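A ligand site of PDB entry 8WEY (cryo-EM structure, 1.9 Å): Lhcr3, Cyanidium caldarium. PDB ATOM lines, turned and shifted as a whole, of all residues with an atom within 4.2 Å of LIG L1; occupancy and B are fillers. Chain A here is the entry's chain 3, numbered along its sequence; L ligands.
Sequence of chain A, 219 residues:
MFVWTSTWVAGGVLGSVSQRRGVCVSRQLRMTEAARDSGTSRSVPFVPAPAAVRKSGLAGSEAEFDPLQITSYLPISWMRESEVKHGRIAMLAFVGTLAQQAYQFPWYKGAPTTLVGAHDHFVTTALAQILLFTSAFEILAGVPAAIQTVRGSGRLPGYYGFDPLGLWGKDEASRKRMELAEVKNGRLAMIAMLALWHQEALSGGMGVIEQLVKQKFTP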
ATOM      1  N   MET A  91       2.471  -3.828  27.070  1.00  0.00           N
ATOM      2  CA  MET A  91       3.769  -3.293  26.566  1.00  0.00           C
ATOM      3  C   MET A  91       4.386  -2.353  27.605  1.00  0.00           C
ATOM      4  O   MET A  91       5.603  -2.464  27.836  1.00  0.00           O
ATOM      5  CB  MET A  91       3.597  -2.580  25.221  1.00  0.00           C
ATOM      6  CG  MET A  91       3.637  -3.543  24.043  1.00  0.00           C
ATOM      7  SD  MET A  91       3.624  -2.725  22.431  1.00  0.00           S
ATOM      8  CE  MET A  91       1.958  -2.084  22.374  1.00  0.00           C
ATOM      9  N   LEU A  92       3.582  -1.473  28.215  1.00  0.00           N
ATOM     10  CA  LEU A  92       4.021  -0.589  29.340  1.00  0.00           C
ATOM     11  C   LEU A  92       4.329  -1.437  30.581  1.00  0.00           C
ATOM     12  O   LEU A  92       5.271  -1.084  31.310  1.00  0.00           O
ATOM     13  CB  LEU A  92       2.932   0.446  29.653  1.00  0.00           C
ATOM     14  CG  LEU A  92       2.651   1.515  28.600  1.00  0.00           C
ATOM     15  CD1 LEU A  92       1.439   2.338  29.000  1.00  0.00           C
ATOM     16  CD2 LEU A  92       3.856   2.406  28.383  1.00  0.00           C
ATOM     17  N   PHE A  94       5.442  -4.618  30.730  1.00  0.00           N
ATOM     18  CA  PHE A  94       6.673  -5.425  30.516  1.00  0.00           C
ATOM     19  C   PHE A  94       7.925  -4.577  30.797  1.00  0.00           C
ATOM     20  O   PHE A  94       8.791  -5.037  31.564  1.00  0.00           O
ATOM     21  CB  PHE A  94       6.719  -6.002  29.092  1.00  0.00           C
ATOM     22  CG  PHE A  94       7.952  -6.812  28.811  1.00  0.00           C
ATOM     23  CD1 PHE A  94       8.107  -8.090  29.328  1.00  0.00           C
ATOM     24  CD2 PHE A  94       8.986  -6.284  28.037  1.00  0.00           C
ATOM     25  CE1 PHE A  94       9.254  -8.827  29.076  1.00  0.00           C
ATOM     26  CE2 PHE A  94      10.128  -7.029  27.787  1.00  0.00           C
ATOM     27  CZ  PHE A  94      10.258  -8.293  28.306  1.00  0.00           C
ATOM     28  N   VAL A  95       8.009  -3.388  30.193  1.00  0.00           N
ATOM     29  CA  VAL A  95       9.151  -2.442  30.379  1.00  0.00           C
ATOM     30  C   VAL A  95       9.033  -1.789  31.767  1.00  0.00           C
ATOM     31  O   VAL A  95      10.073  -1.396  32.314  1.00  0.00           O
ATOM     32  CB  VAL A  95       9.246  -1.387  29.255  1.00  0.00           C
ATOM     33  CG1 VAL A  95       9.289  -2.028  27.880  1.00  0.00           C
ATOM     34  CG2 VAL A  95       8.144  -0.343  29.335  1.00  0.00           C
ATOM     35  N   PHE A 162      -3.432  10.252  19.180  1.00  0.00           N
ATOM     36  CA  PHE A 162      -2.176  10.493  19.933  1.00  0.00           C
ATOM     37  C   PHE A 162      -0.977  10.238  19.014  1.00  0.00           C
ATOM     38  O   PHE A 162      -0.537   9.072  18.895  1.00  0.00           O
ATOM     39  CB  PHE A 162      -2.122   9.633  21.202  1.00  0.00           C
ATOM     40  CG  PHE A 162      -0.838   9.739  21.995  1.00  0.00           C
ATOM     41  CD1 PHE A 162      -0.313  10.978  22.346  1.00  0.00           C
ATOM     42  CD2 PHE A 162      -0.155   8.604  22.415  1.00  0.00           C
ATOM     43  CE1 PHE A 162       0.857  11.078  23.083  1.00  0.00           C
ATOM     44  CE2 PHE A 162       1.015   8.704  23.152  1.00  0.00           C
ATOM     45  CZ  PHE A 162       1.518   9.935  23.481  1.00  0.00           C
ATOM     46  N   ASP A 163      -0.494  11.296  18.359  1.00  0.00           N
ATOM     47  CA  ASP A 163       0.738  11.294  17.534  1.00  0.00           C
ATOM     48  C   ASP A 163       1.326  12.707  17.529  1.00  0.00           C
ATOM     49  O   ASP A 163       1.247  13.409  16.528  1.00  0.00           O
ATOM     50  CB  ASP A 163       0.441  10.734  16.142  1.00  0.00           C
ATOM     51  CG  ASP A 163       1.659  10.295  15.339  1.00  0.00           C
ATOM     52  OD1 ASP A 163       2.656   9.858  15.958  1.00  0.00           O
ATOM     53  OD2 ASP A 163       1.614  10.388  14.098  1.00  0.00           O
ATOM     54  N   PRO A 164       1.883  13.183  18.669  1.00  0.00           N
ATOM     55  CA  PRO A 164       2.665  14.424  18.701  1.00  0.00           C
ATOM     56  C   PRO A 164       3.754  14.507  17.612  1.00  0.00           C
ATOM     57  O   PRO A 164       3.864  15.534  16.980  1.00  0.00           O
ATOM     58  CB  PRO A 164       3.318  14.408  20.095  1.00  0.00           C
ATOM     59  CG  PRO A 164       2.345  13.618  20.946  1.00  0.00           C
ATOM     60  CD  PRO A 164       1.734  12.597  20.018  1.00  0.00           C
ATOM     61  N   LEU A 165       4.510  13.417  17.440  1.00  0.00           N
ATOM     62  CA  LEU A 165       5.564  13.247  16.401  1.00  0.00           C
ATOM     63  C   LEU A 165       4.905  12.721  15.117  1.00  0.00           C
ATOM     64  O   LEU A 165       3.676  12.562  15.109  1.00  0.00           O
ATOM     65  CB  LEU A 165       6.650  12.305  16.934  1.00  0.00           C
ATOM     66  CG  LEU A 165       7.634  12.897  17.947  1.00  0.00           C
ATOM     67  CD1 LEU A 165       6.919  13.420  19.187  1.00  0.00           C
ATOM     68  CD2 LEU A 165       8.690  11.876  18.336  1.00  0.00           C
ATOM     69  N   LEU A 167       5.579   9.613  13.479  1.00  0.00           N
ATOM     70  CA  LEU A 167       6.197   8.249  13.520  1.00  0.00           C
ATOM     71  C   LEU A 167       5.275   7.212  12.860  1.00  0.00           C
ATOM     72  O   LEU A 167       5.795   6.128  12.513  1.00  0.00           O
ATOM     73  CB  LEU A 167       6.494   7.873  14.967  1.00  0.00           C
ATOM     74  CG  LEU A 167       7.192   8.935  15.819  1.00  0.00           C
ATOM     75  CD1 LEU A 167       7.624   8.365  17.164  1.00  0.00           C
ATOM     76  CD2 LEU A 167       8.395   9.521  15.096  1.00  0.00           C
ATOM     77  N   ASN A 185       3.607  -6.354  18.433  1.00  0.00           N
ATOM     78  CA  ASN A 185       4.413  -5.920  19.613  1.00  0.00           C
ATOM     79  C   ASN A 185       3.551  -6.025  20.883  1.00  0.00           C
ATOM     80  O   ASN A 185       4.118  -6.361  21.944  1.00  0.00           O
ATOM     81  CB  ASN A 185       5.002  -4.520  19.461  1.00  0.00           C
ATOM     82  CG  ASN A 185       6.297  -4.505  18.677  1.00  0.00           C
ATOM     83  OD1 ASN A 185       7.360  -4.759  19.237  1.00  0.00           O
ATOM     84  ND2 ASN A 185       6.214  -4.211  17.395  1.00  0.00           N
ATOM     85  N   LEU A 188       3.089  -9.982  21.718  1.00  0.00           N
ATOM     86  CA  LEU A 188       4.347 -10.555  22.259  1.00  0.00           C
ATOM     87  C   LEU A 188       4.544 -10.097  23.708  1.00  0.00           C
ATOM     88  O   LEU A 188       4.963 -10.934  24.538  1.00  0.00           O
ATOM     89  CB  LEU A 188       5.527 -10.132  21.377  1.00  0.00           C
ATOM     90  CG  LEU A 188       6.859 -10.811  21.675  1.00  0.00           C
ATOM     91  CD1 LEU A 188       6.761 -12.318  21.517  1.00  0.00           C
ATOM     92  CD2 LEU A 188       7.959 -10.246  20.785  1.00  0.00           C
ATOM     93  N   ALA A 189       4.247  -8.819  24.004  1.00  0.00           N
ATOM     94  CA  ALA A 189       4.232  -8.239  25.360  1.00  0.00           C
ATOM     95  C   ALA A 189       3.088  -8.843  26.181  1.00  0.00           C
ATOM     96  O   ALA A 189       3.276  -9.027  27.401  1.00  0.00           O
ATOM     97  CB  ALA A 189       4.120  -6.732  25.279  1.00  0.00           C
ATOM     98  N   ALA A 192       4.313 -12.318  26.997  1.00  0.00           N
ATOM     99  CA  ALA A 192       5.436 -12.077  27.922  1.00  0.00           C
ATOM    100  C   ALA A 192       4.918 -11.898  29.352  1.00  0.00           C
ATOM    101  O   ALA A 192       5.406 -12.600  30.248  1.00  0.00           O
ATOM    102  CB  ALA A 192       6.241 -10.873  27.478  1.00  0.00           C
ATOM    103  N   ALA A 195       3.776 -15.025  31.062  1.00  0.00           N
ATOM    104  CA  ALA A 195       4.976 -15.852  31.349  1.00  0.00           C
ATOM    105  C   ALA A 195       5.691 -15.344  32.610  1.00  0.00           C
ATOM    106  O   ALA A 195       6.068 -16.194  33.438  1.00  0.00           O
ATOM    107  CB  ALA A 195       5.896 -15.849  30.155  1.00  0.00           C
ATOM    108  N   LEU A 196       5.870 -14.029  32.746  1.00  0.00           N
ATOM    109  CA  LEU A 196       6.616 -13.388  33.865  1.00  0.00           C
ATOM    110  C   LEU A 196       5.922 -13.673  35.203  1.00  0.00           C
ATOM    111  O   LEU A 196       6.661 -13.855  36.197  1.00  0.00           O
ATOM    112  CB  LEU A 196       6.734 -11.872  33.626  1.00  0.00           C
ATOM    113  CG  LEU A 196       7.592 -11.424  32.439  1.00  0.00           C
ATOM    114  CD1 LEU A 196       7.870  -9.929  32.525  1.00  0.00           C
ATOM    115  CD2 LEU A 196       8.901 -12.194  32.364  1.00  0.00           C
ATOM    116  N   GLN A 199       6.510 -17.499  35.966  1.00  0.00           N
ATOM    117  CA  GLN A 199       7.950 -17.684  36.273  1.00  0.00           C
ATOM    118  C   GLN A 199       8.250 -17.176  37.693  1.00  0.00           C
ATOM    119  O   GLN A 199       8.920 -17.908  38.446  1.00  0.00           O
ATOM    120  CB  GLN A 199       8.824 -16.989  35.231  1.00  0.00           C
ATOM    121  CG  GLN A 199       8.878 -17.739  33.907  1.00  0.00           C
ATOM    122  CD  GLN A 199       9.470 -16.929  32.773  1.00  0.00           C
ATOM    123  OE1 GLN A 199       9.223 -17.204  31.606  1.00  0.00           O
ATOM    124  NE2 GLN A 199      10.270 -15.930  33.110  1.00  0.00           N
HETATM  125  C1  LIG L   1       7.143   0.312  24.854  1.00  0.00           C
HETATM  126  C2  LIG L   1       6.836  -1.215  24.919  1.00  0.00           C
HETATM  127  C3  LIG L   1       6.564   1.002  23.590  1.00  0.00           C
HETATM  128  C4  LIG L   1       9.262 -10.671  25.210  1.00  0.00           C
HETATM  129  C5  LIG L   1       7.184  -2.072  23.659  1.00  0.00           C
HETATM  130  C6  LIG L   1       5.359   9.186  23.047  1.00  0.00           C
HETATM  131  C7  LIG L   1       4.934   6.238  21.791  1.00  0.00           C
HETATM  132  C8  LIG L   1       4.404   5.691  23.145  1.00  0.00           C
HETATM  133  C9  LIG L   1       5.434   4.778  23.877  1.00  0.00           C
HETATM  134  C10 LIG L   1       7.980  -3.369  23.995  1.00  0.00           C
HETATM  135  C11 LIG L   1       5.357   3.287  23.431  1.00  0.00           C
HETATM  136  C12 LIG L   1       6.714   2.546  23.494  1.00  0.00           C
HETATM  137  C13 LIG L   1      12.979 -11.446  28.530  1.00  0.00           C
HETATM  138  C14 LIG L   1      12.603 -12.889  28.166  1.00  0.00           C
HETATM  139  C15 LIG L   1      13.094 -13.828  29.354  1.00  0.00           C
HETATM  140  C16 LIG L   1       7.351  -6.201  22.196  1.00  0.00           C
HETATM  141  C17 LIG L   1      11.993 -14.042  30.468  1.00  0.00           C
HETATM  142  C18 LIG L   1      10.758 -14.697  29.843  1.00  0.00           C
HETATM  143  C19 LIG L   1      10.242 -13.977  28.624  1.00  0.00           C
HETATM  144  C20 LIG L   1      11.089 -12.973  27.966  1.00  0.00           C
HETATM  145  C21 LIG L   1       9.973 -11.174  23.950  1.00  0.00           C
HETATM  146  C22 LIG L   1      10.603 -12.554  26.533  1.00  0.00           C
HETATM  147  C23 LIG L   1       9.936 -11.153  26.544  1.00  0.00           C
HETATM  148  C24 LIG L   1       7.119  -4.635  24.206  1.00  0.00           C
HETATM  149  C25 LIG L   1      13.372 -13.295  26.896  1.00  0.00           C
HETATM  150  C26 LIG L   1       7.775  -5.927  23.640  1.00  0.00           C
HETATM  151  C27 LIG L   1       7.576  -7.153  24.558  1.00  0.00           C
HETATM  152  C28 LIG L   1       8.302  -8.462  24.110  1.00  0.00           C
HETATM  153  C29 LIG L   1       9.064  -9.128  25.274  1.00  0.00           C
HETATM  154  C30 LIG L   1       8.824 -13.426  28.847  1.00  0.00           C
HETATM  155  C31 LIG L   1       2.148   6.718  20.561  1.00  0.00           C
HETATM  156  C32 LIG L   1       3.436   7.495  20.245  1.00  0.00           C
HETATM  157  C33 LIG L   1       4.330   7.611  21.406  1.00  0.00           C
HETATM  158  C34 LIG L   1       5.299   8.780  21.560  1.00  0.00           C
HETATM  159  C35 LIG L   1       4.805  10.015  20.724  1.00  0.00           C
HETATM  160  C36 LIG L   1       4.378   9.627  19.267  1.00  0.00           C
HETATM  161  C37 LIG L   1       3.189   8.665  19.336  1.00  0.00           C
HETATM  162  O1  LIG L   1       4.010  10.758  18.569  1.00  0.00           O
HETATM  163  C38 LIG L   1       6.713   8.394  21.074  1.00  0.00           C
HETATM  164  O2  LIG L   1      12.491 -14.844  31.465  1.00  0.00           O
HETATM  165  C39 LIG L   1       6.716   0.994  26.173  1.00  0.00           C
HETATM  166  C40 LIG L   1       5.424   4.956  25.399  1.00  0.00           C
HETATM  167 MG1  LG2 L   2      10.154  -4.484  19.238  1.00  0.00          MG
HETATM  168  C1  LG2 L   2       9.782  -3.955  15.849  1.00  0.00           C
HETATM  169  C2  LG2 L   2       9.857  -1.136  19.696  1.00  0.00           C
HETATM  170  C3  LG2 L   2      11.112  -5.001  22.442  1.00  0.00           C
HETATM  171  C4  LG2 L   2      10.775  -8.054  18.493  1.00  0.00           C
HETATM  172  N1  LG2 L   2       9.904  -2.829  18.011  1.00  0.00           N
HETATM  173  C5  LG2 L   2       9.654  -2.772  16.750  1.00  0.00           C
HETATM  174  C6  LG2 L   2       9.296  -1.429  16.161  1.00  0.00           C
HETATM  175  C7  LG2 L   2       9.343  -0.546  17.418  1.00  0.00           C
HETATM  176  C8  LG2 L   2       9.728  -1.579  18.438  1.00  0.00           C
HETATM  177  C9  LG2 L   2      10.377   0.575  17.278  1.00  0.00           C
HETATM  178  C10 LG2 L   2       7.924  -1.402  15.478  1.00  0.00           C
HETATM  179  C11 LG2 L   2       7.955  -0.538  14.219  1.00  0.00           C
HETATM  180  N2  LG2 L   2      10.443  -3.242  20.842  1.00  0.00           N
HETATM  181  C12 LG2 L   2      10.236  -1.930  20.868  1.00  0.00           C
HETATM  182  C13 LG2 L   2      10.469  -1.278  22.187  1.00  0.00           C
HETATM  183  C14 LG2 L   2      10.862  -2.434  23.038  1.00  0.00           C
HETATM  184  C15 LG2 L   2      10.798  -3.601  22.084  1.00  0.00           C
HETATM  185  C16 LG2 L   2      10.338   0.173  22.570  1.00  0.00           C
HETATM  186  C17 LG2 L   2      11.194  -2.300  24.489  1.00  0.00           C
HETATM  187  C18 LG2 L   2      11.549  -3.260  25.346  1.00  0.00           C
HETATM  188  N3  LG2 L   2      10.813  -6.170  20.226  1.00  0.00           N
HETATM  189  C19 LG2 L   2      11.118  -6.166  21.533  1.00  0.00           C
HETATM  190  C20 LG2 L   2      11.517  -7.494  22.093  1.00  0.00           C
HETATM  191  C21 LG2 L   2      11.407  -8.392  20.922  1.00  0.00           C
HETATM  192  C22 LG2 L   2      10.966  -7.474  19.842  1.00  0.00           C
HETATM  193  C23 LG2 L   2      11.926  -7.872  23.486  1.00  0.00           C
HETATM  194  C24 LG2 L   2      11.687  -9.880  20.840  1.00  0.00           C
HETATM  195  C25 LG2 L   2      13.000 -10.085  20.115  1.00  0.00           C
HETATM  196  N4  LG2 L   2      10.256  -5.764  17.648  1.00  0.00           N
HETATM  197  C26 LG2 L   2      10.498  -7.150  17.373  1.00  0.00           C
HETATM  198  C27 LG2 L   2      10.496  -7.532  15.934  1.00  0.00           C
HETATM  199  C28 LG2 L   2      10.217  -6.207  15.326  1.00  0.00           C
HETATM  200  C29 LG2 L   2      10.111  -5.287  16.365  1.00  0.00           C
HETATM  201  C30 LG2 L   2      10.705  -8.794  15.135  1.00  0.00           C
HETATM  202  C31 LG2 L   2       9.999  -5.465  14.044  1.00  0.00           C
HETATM  203  O1  LG2 L   2      10.043  -5.985  12.874  1.00  0.00           O
HETATM  204  C32 LG2 L   2       9.747  -4.032  14.360  1.00  0.00           C
HETATM  205  C33 LG2 L   2      10.840  -3.185  13.760  1.00  0.00           C
HETATM  206  O2  LG2 L   2      12.004  -3.299  14.115  1.00  0.00           O
HETATM  207  O3  LG2 L   2      10.509  -2.201  12.726  1.00  0.00           O
HETATM  208  C34 LG2 L   2      11.430  -1.892  11.678  1.00  0.00           C
HETATM  209 MG1  LG3 L   3       1.042   3.215  19.860  1.00  0.00          MG
HETATM  210  C1  LG3 L   3      -1.340   5.134  18.252  1.00  0.00           C
HETATM  211  C2  LG3 L   3       2.177   2.255  16.811  1.00  0.00           C
HETATM  212  C3  LG3 L   3       3.063   1.037  21.493  1.00  0.00           C
HETATM  213  C4  LG3 L   3      -0.592   4.130  23.046  1.00  0.00           C
HETATM  214  N1  LG3 L   3       0.513   3.575  17.898  1.00  0.00           N
HETATM  215  C5  LG3 L   3      -0.357   4.391  17.421  1.00  0.00           C
HETATM  216  C6  LG3 L   3      -0.348   4.620  15.934  1.00  0.00           C
HETATM  217  C7  LG3 L   3       0.741   3.651  15.482  1.00  0.00           C
HETATM  218  C8  LG3 L   3       1.169   3.119  16.824  1.00  0.00           C
HETATM  219  C9  LG3 L   3       0.188   2.562  14.561  1.00  0.00           C
HETATM  220  C10 LG3 L   3       0.048   6.070  15.600  1.00  0.00           C
HETATM  221  C11 LG3 L   3       1.045   6.785  16.539  1.00  0.00           C
HETATM  222  C12 LG3 L   3       2.479   6.420  16.223  1.00  0.00           C
HETATM  223  O1  LG3 L   3       2.999   6.869  15.215  1.00  0.00           O
HETATM  224  O2  LG3 L   3       3.223   5.528  17.109  1.00  0.00           O
HETATM  225  N2  LG3 L   3       2.410   1.818  19.243  1.00  0.00           N
HETATM  226  C13 LG3 L   3       2.786   1.596  17.984  1.00  0.00           C
HETATM  227  C14 LG3 L   3       3.914   0.657  17.808  1.00  0.00           C
HETATM  228  C15 LG3 L   3       4.207   0.264  19.208  1.00  0.00           C
HETATM  229  C16 LG3 L   3       3.204   1.058  20.014  1.00  0.00           C
HETATM  230  C17 LG3 L   3       4.612   0.188  16.556  1.00  0.00           C
HETATM  231  C18 LG3 L   3       5.326  -0.674  19.530  1.00  0.00           C
HETATM  232  C19 LG3 L   3       5.808  -0.956  20.721  1.00  0.00           C
HETATM  233  N3  LG3 L   3       1.143   2.662  21.851  1.00  0.00           N
HETATM  234  C20 LG3 L   3       2.092   1.815  22.304  1.00  0.00           C
HETATM  235  C21 LG3 L   3       2.120   1.715  23.799  1.00  0.00           C
HETATM  236  C22 LG3 L   3       1.048   2.629  24.232  1.00  0.00           C
HETATM  237  C23 LG3 L   3       0.526   3.155  22.950  1.00  0.00           C
HETATM  238  C24 LG3 L   3       3.000   0.897  24.702  1.00  0.00           C
HETATM  239  C25 LG3 L   3       0.587   2.947  25.633  1.00  0.00           C
HETATM  240  C26 LG3 L   3       1.120   4.322  25.997  1.00  0.00           C
HETATM  241  N4  LG3 L   3      -0.536   4.295  20.575  1.00  0.00           N
HETATM  242  C27 LG3 L   3      -1.138   4.679  21.816  1.00  0.00           C
HETATM  243  C28 LG3 L   3      -2.310   5.594  21.722  1.00  0.00           C
HETATM  244  C29 LG3 L   3      -2.378   5.763  20.247  1.00  0.00           C
HETATM  245  C30 LG3 L   3      -1.355   4.993  19.708  1.00  0.00           C
HETATM  246  C31 LG3 L   3      -3.253   6.254  22.703  1.00  0.00           C
HETATM  247  C32 LG3 L   3      -3.094   6.418  19.121  1.00  0.00           C
HETATM  248  O3  LG3 L   3      -4.115   7.196  19.236  1.00  0.00           O
HETATM  249  C33 LG3 L   3      -2.470   5.993  17.842  1.00  0.00           C
HETATM  250  C34 LG3 L   3      -3.436   5.137  17.081  1.00  0.00           C
HETATM  251  O4  LG3 L   3      -3.773   4.062  17.543  1.00  0.00           O
HETATM  252  O5  LG3 L   3      -3.970   5.533  15.793  1.00  0.00           O
HETATM  253  C35 LG3 L   3      -4.611   4.549  14.974  1.00  0.00           C
HETATM  254  C36 LG3 L   3       4.649   5.446  17.022  1.00  0.00           C
HETATM  255  C37 LG3 L   3       5.218   4.360  17.905  1.00  0.00           C
HETATM  256  C38 LG3 L   3       6.534   4.045  17.931  1.00  0.00           C
HETATM  257  C39 LG3 L   3       7.577   4.732  17.079  1.00  0.00           C
HETATM  258  C40 LG3 L   3       7.004   2.944  18.847  1.00  0.00           C
HETATM  259  C41 LG3 L   3       7.329   3.424  20.262  1.00  0.00           C
HETATM  260  C42 LG3 L   3       8.465   4.443  20.287  1.00  0.00           C
HETATM  261 MG1  LG4 L   4       8.656 -19.910  30.380  1.00  0.00          MG
HETATM  262  C1  LG4 L   4       9.849 -21.357  33.302  1.00  0.00           C
HETATM  263  C2  LG4 L   4      11.832 -18.984  29.638  1.00  0.00           C
HETATM  264  C3  LG4 L   4       7.369 -18.203  27.751  1.00  0.00           C
HETATM  265  C4  LG4 L   4       5.225 -20.651  31.568  1.00  0.00           C
HETATM  266  N1  LG4 L   4      10.507 -20.094  31.303  1.00  0.00           N
HETATM  267  C5  LG4 L   4      10.848 -20.723  32.377  1.00  0.00           C
HETATM  268  C6  LG4 L   4      12.330 -20.798  32.682  1.00  0.00           C
HETATM  269  C7  LG4 L   4      12.927 -20.017  31.517  1.00  0.00           C
HETATM  270  C8  LG4 L   4      11.668 -19.675  30.772  1.00  0.00           C
HETATM  271  C9  LG4 L   4      13.670 -18.768  31.991  1.00  0.00           C
HETATM  272  C10 LG4 L   4      12.961 -22.202  32.822  1.00  0.00           C
HETATM  273  C11 LG4 L   4      13.031 -23.140  31.600  1.00  0.00           C
HETATM  274  C12 LG4 L   4      11.773 -23.201  30.774  1.00  0.00           C
HETATM  275  O1  LG4 L   4      10.761 -23.748  31.204  1.00  0.00           O
HETATM  276  O2  LG4 L   4      11.747 -22.630  29.438  1.00  0.00           O
HETATM  277  N2  LG4 L   4       9.478 -18.745  28.915  1.00  0.00           N
HETATM  278  C13 LG4 L   4      10.775 -18.512  28.722  1.00  0.00           C
HETATM  279  C14 LG4 L   4      11.108 -17.753  27.486  1.00  0.00           C
HETATM  280  C15 LG4 L   4       9.771 -17.510  26.899  1.00  0.00           C
HETATM  281  C16 LG4 L   4       8.840 -18.173  27.878  1.00  0.00           C
HETATM  282  C17 LG4 L   4      12.458 -17.335  26.952  1.00  0.00           C
HETATM  283  C18 LG4 L   4       9.571 -16.754  25.617  1.00  0.00           C
HETATM  284  C19 LG4 L   4       8.431 -16.473  25.013  1.00  0.00           C
HETATM  285  N3  LG4 L   4       6.707 -19.493  29.825  1.00  0.00           N
HETATM  286  C20 LG4 L   4       6.402 -18.839  28.685  1.00  0.00           C
HETATM  287  C21 LG4 L   4       4.954 -18.762  28.372  1.00  0.00           C
HETATM  288  C22 LG4 L   4       4.326 -19.481  29.495  1.00  0.00           C
HETATM  289  C23 LG4 L   4       5.501 -19.888  30.322  1.00  0.00           C
HETATM  290  C24 LG4 L   4       4.193 -18.139  27.227  1.00  0.00           C
HETATM  291  C25 LG4 L   4       2.849 -19.729  29.724  1.00  0.00           C
HETATM  292  C26 LG4 L   4       2.544 -21.127  29.242  1.00  0.00           C
HETATM  293  N4  LG4 L   4       7.689 -20.723  31.988  1.00  0.00           N
HETATM  294  C27 LG4 L   4       6.353 -21.065  32.400  1.00  0.00           C
HETATM  295  C28 LG4 L   4       6.243 -21.842  33.667  1.00  0.00           C
HETATM  296  C29 LG4 L   4       7.690 -21.951  34.019  1.00  0.00           C
HETATM  297  C30 LG4 L   4       8.409 -21.296  33.022  1.00  0.00           C
HETATM  298  C31 LG4 L   4       5.129 -22.426  34.491  1.00  0.00           C
HETATM  299  C32 LG4 L   4       8.664 -22.470  35.005  1.00  0.00           C
HETATM  300  O3  LG4 L   4       8.369 -23.140  36.064  1.00  0.00           O
HETATM  301  C33 LG4 L   4      10.032 -22.113  34.558  1.00  0.00           C
HETATM  302  C34 LG4 L   4      10.737 -21.302  35.616  1.00  0.00           C
HETATM  303  O4  LG4 L   4      10.250 -20.281  36.063  1.00  0.00           O
HETATM  304  O5  LG4 L   4      12.033 -21.741  36.117  1.00  0.00           O
HETATM  305  C35 LG4 L   4      12.182 -22.297  37.422  1.00  0.00           C
HETATM  306  C36 LG4 L   4      12.589 -23.152  28.410  1.00  0.00           C
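The backbone nitrogen of Pro 164 sits close to an oxygen (O1) of LIG L1, at 3.2 Å. Merely in contact with LIG L1: Met 91, Leu 92, Phe 94, Val 95, Phe 162, Asn 185, Leu 188, Ala 189, Ala 192 and Leu 196. Of the 16 residues printed, 14 come within 4 Å of LIG L1. Along chain A the residues within 4 Å of LIG L1 span positions 91 to 199. The nearest printed residue that does not touch LIG L1 is Leu 167 (4.01 Å).
The backbone NH of Phe 162 sits at hydrogen-bond distance from an oxygen (O3) of LG3 L3, at 3.1 Å. O1 of LIG L1 lies within hydrogen-bond range of OD1 of Asp 163 (3.1 Å). The backbone NH (N) of Leu 165 is in hydrogen-bond range of an oxygen (O1) of LIG L1 (2.9 Å). An oxygen (O2) of LIG L1 lies within hydrogen-bond range of the side-chain amide nitrogen (NE2) of Gln 199 (3.0 Å).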
